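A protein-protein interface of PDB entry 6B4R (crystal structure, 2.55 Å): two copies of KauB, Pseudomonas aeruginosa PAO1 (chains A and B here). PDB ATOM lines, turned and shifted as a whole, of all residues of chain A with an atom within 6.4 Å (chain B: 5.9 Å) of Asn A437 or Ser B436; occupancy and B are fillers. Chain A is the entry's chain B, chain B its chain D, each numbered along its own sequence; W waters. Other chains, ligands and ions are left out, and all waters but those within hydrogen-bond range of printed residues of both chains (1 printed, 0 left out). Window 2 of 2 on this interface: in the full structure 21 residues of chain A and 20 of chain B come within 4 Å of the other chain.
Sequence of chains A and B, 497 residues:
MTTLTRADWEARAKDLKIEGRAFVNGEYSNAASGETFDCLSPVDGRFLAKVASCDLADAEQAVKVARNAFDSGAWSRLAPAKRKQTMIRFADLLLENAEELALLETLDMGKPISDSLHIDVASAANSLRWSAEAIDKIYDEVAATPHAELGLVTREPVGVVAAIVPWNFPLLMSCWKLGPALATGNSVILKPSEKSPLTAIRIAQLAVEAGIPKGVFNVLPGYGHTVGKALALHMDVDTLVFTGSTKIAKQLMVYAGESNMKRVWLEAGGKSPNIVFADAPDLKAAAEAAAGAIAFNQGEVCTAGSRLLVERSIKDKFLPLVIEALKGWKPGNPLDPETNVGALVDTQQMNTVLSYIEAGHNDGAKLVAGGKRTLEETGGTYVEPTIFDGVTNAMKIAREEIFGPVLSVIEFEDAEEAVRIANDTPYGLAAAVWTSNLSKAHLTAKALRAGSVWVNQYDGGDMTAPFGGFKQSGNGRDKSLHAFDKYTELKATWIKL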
ATOM      1  N   ASP A 279     -20.384  19.835 -19.790  1.00  0.00           N
ATOM      2  CA  ASP A 279     -20.951  19.445 -18.505  1.00  0.00           C
ATOM      3  C   ASP A 279     -19.921  19.459 -17.377  1.00  0.00           C
ATOM      4  O   ASP A 279     -19.980  18.640 -16.459  1.00  0.00           O
ATOM      5  CB  ASP A 279     -21.626  18.071 -18.607  1.00  0.00           C
ATOM      6  CG  ASP A 279     -20.668  16.976 -19.048  1.00  0.00           C
ATOM      7  OD1 ASP A 279     -19.554  17.301 -19.510  1.00  0.00           O
ATOM      8  OD2 ASP A 279     -21.036  15.787 -18.939  1.00  0.00           O
ATOM      9  N   THR A 435     -15.228  17.424 -16.616  1.00  0.00           N
ATOM     10  CA  THR A 435     -16.584  16.917 -16.798  1.00  0.00           C
ATOM     11  C   THR A 435     -17.141  16.385 -15.484  1.00  0.00           C
ATOM     12  O   THR A 435     -16.386  16.039 -14.577  1.00  0.00           O
ATOM     13  CB  THR A 435     -16.642  15.805 -17.863  1.00  0.00           C
ATOM     14  OG1 THR A 435     -17.973  15.279 -17.941  1.00  0.00           O
ATOM     15  CG2 THR A 435     -15.684  14.684 -17.516  1.00  0.00           C
ATOM     16  N   SER A 436     -18.464  16.325 -15.386  1.00  0.00           N
ATOM     17  CA  SER A 436     -19.119  15.838 -14.177  1.00  0.00           C
ATOM     18  C   SER A 436     -19.647  14.421 -14.369  1.00  0.00           C
ATOM     19  O   SER A 436     -20.157  13.807 -13.434  1.00  0.00           O
ATOM     20  CB  SER A 436     -20.262  16.769 -13.767  1.00  0.00           C
ATOM     21  OG  SER A 436     -21.308  16.754 -14.725  1.00  0.00           O
ATOM     22  N   ASN A 437     -19.516  13.908 -15.589  1.00  0.00           N
ATOM     23  CA  ASN A 437     -19.990  12.566 -15.906  1.00  0.00           C
ATOM     24  C   ASN A 437     -18.954  11.494 -15.582  1.00  0.00           C
ATOM     25  O   ASN A 437     -17.787  11.615 -15.952  1.00  0.00           O
ATOM     26  CB  ASN A 437     -20.417  12.476 -17.372  1.00  0.00           C
ATOM     27  CG  ASN A 437     -20.981  11.116 -17.731  1.00  0.00           C
ATOM     28  OD1 ASN A 437     -20.448  10.416 -18.595  1.00  0.00           O
ATOM     29  ND2 ASN A 437     -22.057  10.724 -17.055  1.00  0.00           N
ATOM     30  N   LEU A 438     -19.398  10.447 -14.895  1.00  0.00           N
ATOM     31  CA  LEU A 438     -18.523   9.375 -14.430  1.00  0.00           C
ATOM     32  C   LEU A 438     -17.830   8.640 -15.574  1.00  0.00           C
ATOM     33  O   LEU A 438     -16.599   8.584 -15.636  1.00  0.00           O
ATOM     34  CB  LEU A 438     -19.318   8.376 -13.587  1.00  0.00           C
ATOM     35  CG  LEU A 438     -18.574   7.123 -13.126  1.00  0.00           C
ATOM     36  CD1 LEU A 438     -17.549   7.470 -12.058  1.00  0.00           C
ATOM     37  CD2 LEU A 438     -19.549   6.069 -12.624  1.00  0.00           C
ATOM     38  N   SER A 439     -18.627   8.076 -16.474  1.00  0.00           N
ATOM     39  CA  SER A 439     -18.097   7.291 -17.583  1.00  0.00           C
ATOM     40  C   SER A 439     -17.230   8.117 -18.527  1.00  0.00           C
ATOM     41  O   SER A 439     -16.171   7.661 -18.957  1.00  0.00           O
ATOM     42  CB  SER A 439     -19.234   6.621 -18.361  1.00  0.00           C
ATOM     43  OG  SER A 439     -19.912   5.673 -17.556  1.00  0.00           O
ATOM     44  N   LYS A 440     -17.674   9.329 -18.849  1.00  0.00           N
ATOM     45  CA  LYS A 440     -16.934  10.175 -19.780  1.00  0.00           C
ATOM     46  C   LYS A 440     -15.583  10.597 -19.205  1.00  0.00           C
ATOM     47  O   LYS A 440     -14.596  10.686 -19.932  1.00  0.00           O
ATOM     48  CB  LYS A 440     -17.753  11.401 -20.196  1.00  0.00           C
ATOM     49  CG  LYS A 440     -17.083  12.241 -21.280  1.00  0.00           C
ATOM     50  CD  LYS A 440     -18.056  13.201 -21.950  1.00  0.00           C
ATOM     51  CE  LYS A 440     -18.590  14.235 -20.974  1.00  0.00           C
ATOM     52  NZ  LYS A 440     -19.526  15.187 -21.636  1.00  0.00           N
ATOM     53  N   ALA A 441     -15.546  10.846 -17.899  1.00  0.00           N
ATOM     54  CA  ALA A 441     -14.309  11.247 -17.234  1.00  0.00           C
ATOM     55  C   ALA A 441     -13.251  10.150 -17.301  1.00  0.00           C
ATOM     56  O   ALA A 441     -12.110  10.404 -17.691  1.00  0.00           O
ATOM     57  CB  ALA A 441     -14.584  11.632 -15.788  1.00  0.00           C
ATOM     58  N   HIS A 442     -13.636   8.932 -16.930  1.00  0.00           N
ATOM     59  CA  HIS A 442     -12.702   7.808 -16.906  1.00  0.00           C
ATOM     60  C   HIS A 442     -12.314   7.323 -18.303  1.00  0.00           C
ATOM     61  O   HIS A 442     -11.143   7.055 -18.563  1.00  0.00           O
ATOM     62  CB  HIS A 442     -13.263   6.644 -16.080  1.00  0.00           C
ATOM     63  CG  HIS A 442     -13.251   6.888 -14.602  1.00  0.00           C
ATOM     64  ND1 HIS A 442     -12.108   6.780 -13.838  1.00  0.00           N
ATOM     65  CD2 HIS A 442     -14.244   7.227 -13.746  1.00  0.00           C
ATOM     66  CE1 HIS A 442     -12.396   7.048 -12.577  1.00  0.00           C
ATOM     67  NE2 HIS A 442     -13.686   7.321 -12.494  1.00  0.00           N
ATOM     68  N   ASP B 279     -30.142  10.543 -11.195  1.00  0.00           N
ATOM     69  CA  ASP B 279     -29.304  10.753 -12.371  1.00  0.00           C
ATOM     70  C   ASP B 279     -28.648   9.467 -12.874  1.00  0.00           C
ATOM     71  O   ASP B 279     -27.614   9.512 -13.539  1.00  0.00           O
ATOM     72  CB  ASP B 279     -28.244  11.832 -12.110  1.00  0.00           C
ATOM     73  CG  ASP B 279     -27.388  11.538 -10.889  1.00  0.00           C
ATOM     74  OD1 ASP B 279     -27.422  10.392 -10.391  1.00  0.00           O
ATOM     75  OD2 ASP B 279     -26.672  12.456 -10.433  1.00  0.00           O
ATOM     76  N   ALA B 280     -29.251   8.329 -12.546  1.00  0.00           N
ATOM     77  CA  ALA B 280     -28.773   7.042 -13.036  1.00  0.00           C
ATOM     78  C   ALA B 280     -28.796   7.016 -14.561  1.00  0.00           C
ATOM     79  O   ALA B 280     -29.754   7.486 -15.177  1.00  0.00           O
ATOM     80  CB  ALA B 280     -29.618   5.913 -12.466  1.00  0.00           C
ATOM     81  N   PRO B 281     -27.730   6.472 -15.173  1.00  0.00           N
ATOM     82  CA  PRO B 281     -27.564   6.419 -16.633  1.00  0.00           C
ATOM     83  C   PRO B 281     -28.752   5.768 -17.337  1.00  0.00           C
ATOM     84  O   PRO B 281     -29.255   6.310 -18.321  1.00  0.00           O
ATOM     85  CB  PRO B 281     -26.313   5.553 -16.806  1.00  0.00           C
ATOM     86  CG  PRO B 281     -25.547   5.745 -15.545  1.00  0.00           C
ATOM     87  CD  PRO B 281     -26.583   5.878 -14.465  1.00  0.00           C
ATOM     88  N   TRP B 434     -25.981   3.828  -8.071  1.00  0.00           N
ATOM     89  CA  TRP B 434     -26.367   4.088  -9.453  1.00  0.00           C
ATOM     90  C   TRP B 434     -26.468   5.587  -9.726  1.00  0.00           C
ATOM     91  O   TRP B 434     -27.433   6.238  -9.330  1.00  0.00           O
ATOM     92  CB  TRP B 434     -27.691   3.392  -9.776  1.00  0.00           C
ATOM     93  CG  TRP B 434     -27.626   1.896  -9.655  1.00  0.00           C
ATOM     94  CD1 TRP B 434     -27.683   1.160  -8.504  1.00  0.00           C
ATOM     95  CD2 TRP B 434     -27.492   0.955 -10.726  1.00  0.00           C
ATOM     96  NE1 TRP B 434     -27.591  -0.180  -8.794  1.00  0.00           N
ATOM     97  CE2 TRP B 434     -27.474  -0.332 -10.152  1.00  0.00           C
ATOM     98  CE3 TRP B 434     -27.388   1.076 -12.116  1.00  0.00           C
ATOM     99  CZ2 TRP B 434     -27.355  -1.490 -10.917  1.00  0.00           C
ATOM    100  CZ3 TRP B 434     -27.271  -0.076 -12.875  1.00  0.00           C
ATOM    101  CH2 TRP B 434     -27.256  -1.341 -12.274  1.00  0.00           C
ATOM    102  N   THR B 435     -25.461   6.127 -10.405  1.00  0.00           N
ATOM    103  CA  THR B 435     -25.406   7.552 -10.707  1.00  0.00           C
ATOM    104  C   THR B 435     -24.448   7.828 -11.859  1.00  0.00           C
ATOM    105  O   THR B 435     -23.515   7.063 -12.099  1.00  0.00           O
ATOM    106  CB  THR B 435     -24.958   8.373  -9.484  1.00  0.00           C
ATOM    107  OG1 THR B 435     -24.678   9.719  -9.885  1.00  0.00           O
ATOM    108  CG2 THR B 435     -23.708   7.774  -8.874  1.00  0.00           C
ATOM    109  N   SER B 436     -24.686   8.927 -12.567  1.00  0.00           N
ATOM    110  CA  SER B 436     -23.843   9.308 -13.693  1.00  0.00           C
ATOM    111  C   SER B 436     -22.892  10.431 -13.300  1.00  0.00           C
ATOM    112  O   SER B 436     -22.052  10.851 -14.095  1.00  0.00           O
ATOM    113  CB  SER B 436     -24.701   9.745 -14.881  1.00  0.00           C
ATOM    114  OG  SER B 436     -25.415  10.932 -14.578  1.00  0.00           O
ATOM    115  N   ASN B 437     -23.031  10.919 -12.073  1.00  0.00           N
ATOM    116  CA  ASN B 437     -22.182  11.996 -11.583  1.00  0.00           C
ATOM    117  C   ASN B 437     -20.862  11.466 -11.033  1.00  0.00           C
ATOM    118  O   ASN B 437     -20.847  10.590 -10.167  1.00  0.00           O
ATOM    119  CB  ASN B 437     -22.911  12.822 -10.522  1.00  0.00           C
ATOM    120  CG  ASN B 437     -22.129  14.051 -10.107  1.00  0.00           C
ATOM    121  OD1 ASN B 437     -21.449  14.055  -9.080  1.00  0.00           O
ATOM    122  ND2 ASN B 437     -22.215  15.102 -10.911  1.00  0.00           N
ATOM    123  N   LEU B 438     -19.760  12.009 -11.543  1.00  0.00           N
ATOM    124  CA  LEU B 438     -18.420  11.550 -11.184  1.00  0.00           C
ATOM    125  C   LEU B 438     -18.123  11.653  -9.690  1.00  0.00           C
ATOM    126  O   LEU B 438     -17.747  10.666  -9.057  1.00  0.00           O
ATOM    127  CB  LEU B 438     -17.363  12.325 -11.974  1.00  0.00           C
ATOM    128  CG  LEU B 438     -15.908  12.020 -11.610  1.00  0.00           C
ATOM    129  CD1 LEU B 438     -15.570  10.574 -11.935  1.00  0.00           C
ATOM    130  CD2 LEU B 438     -14.966  12.974 -12.323  1.00  0.00           C
ATOM    131  N   ASN B 456     -22.953   1.567 -10.856  1.00  0.00           N
ATOM    132  CA  ASN B 456     -23.680   1.370 -12.112  1.00  0.00           C
ATOM    133  C   ASN B 456     -23.810  -0.095 -12.530  1.00  0.00           C
ATOM    134  O   ASN B 456     -23.925  -0.402 -13.716  1.00  0.00           O
ATOM    135  CB  ASN B 456     -23.066   2.202 -13.244  1.00  0.00           C
ATOM    136  CG  ASN B 456     -23.136   3.693 -12.972  1.00  0.00           C
ATOM    137  OD1 ASN B 456     -23.922   4.147 -12.140  1.00  0.00           O
ATOM    138  ND2 ASN B 456     -22.316   4.464 -13.679  1.00  0.00           N
HETATM  139  O   HOH W   1     -18.551  15.018 -10.739  1.00  0.00           O
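Water W1 lies within hydrogen-bond range of the backbone NH of Leu B438 (3.3 Å), the backbone carbonyl oxygen of Ser A436 (3.4 Å) and the side-chain amide oxygen of Asn B437 (3.5 Å).
Of the 9 printed residues of chain B, 4 touch a printed residue of chain A.
Printed residues of chain B that touch a printed residue of chain A: Ser B436, Asn B437, Leu B438 and Asn B456.
Hydrophobic or aromatic side chains of chain B that line the printed part of chain A: Leu B438.
Along chain B the printed residues that touch a printed residue of chain A span positions 436 to 456.
Of the 9 printed residues of chain A, 5 touch a printed residue of chain B.
Hydrophobic or aromatic side chains of chain A within 4 Å of the printed part of chain B: Leu A438, Ala A441 and His A442.
Along chain A the printed residues that touch a printed residue of chain B span positions 436 to 442.
Among the printed residues, no Asp or Glu carboxylate lies within 4 Å of a Lys or Arg side-chain nitrogen of the other chain.
The backbone carbonyl oxygen (O) of Ser A436 is in hydrogen-bond range of the backbone NH (N) of Leu B438, at 2.6 Å.
O of Ser B436 is in hydrogen-bond range of ND2 of Asn A437 (3.0 Å).
The backbone carbonyl oxygen of Ser B436 lies within hydrogen-bond range of the backbone NH of Leu A438 (2.8 Å).
Ser B436 touches its own counterpart, Ser A436.
Ser A436 touches Asn B437, and with the chains exchanged Asn A437 touches Ser B436.
Ser A436 touches Leu B438, and with the chains exchanged Leu A438 touches Ser B436.
Leu B438 touches its own counterpart, Leu A438.
5 positions are printed for both chains.
Of the 9 pairs that touch across the chains among the printed residues, 6 have their exchanged pair printed and touching as well.
The backbone carbonyl oxygen of Asp A279 sits at hydrogen-bond distance from the side-chain hydroxyl of Ser A436 (2.9 Å).
The side-chain hydroxyl (OG1) of Thr A435 sits at hydrogen-bond distance from the backbone NH (N) of Asn A437.
OD1 of Asn A437 sits at hydrogen-bond distance from N of Lys A440, at 3.0 Å.
The backbone carbonyl oxygen (O) of Asp B279 sits at hydrogen-bond distance from the side-chain hydroxyl (OG) of Ser B436.
OG1 of Thr B435 is in hydrogen-bond range of N of Asn B437 (3.0 Å).
The backbone carbonyl oxygen (O) of Thr B435 lies close to the side-chain amide oxygen (OD1) of Asn B456.
Printed residues of chain B within 4 Å of Ser A436: Ser B436 (3.6 Å), Asn B437 (3.3 Å) and Leu B438 (2.6 Å).
Asn A437 touches one residue of chain B.
Of the printed residues of chain B, Ala A441 touches Leu B438.
Ala B280 touches none of the printed residues of chain A.
Printed residues of chain A within 4 Å of Ser B436: Ser A436 (3.6 Å), Asn A437 (3.0 Å) and Leu A438 (2.8 Å).
Of the printed residues of chain A, Asn B437 touches Ser A436 (3.3 Å).
Of the printed residues of chain A, Asn B456 touches Leu A438.
The nearest residue of chain B that does not touch Asn A437 is Leu B438 (4.03 Å).
Among the printed residues, merely in contact across the chains: Ser A436 with Ser B436 (3.6 Å), Ser A436 with Asn B437 (3.3 Å), Leu A438 with Leu B438 (3.7 Å), Leu A438 with Asn B456 (3.4 Å), Ala A441 with Leu B438 (3.7 Å) and His A442 with Leu B438 (3.8 Å).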
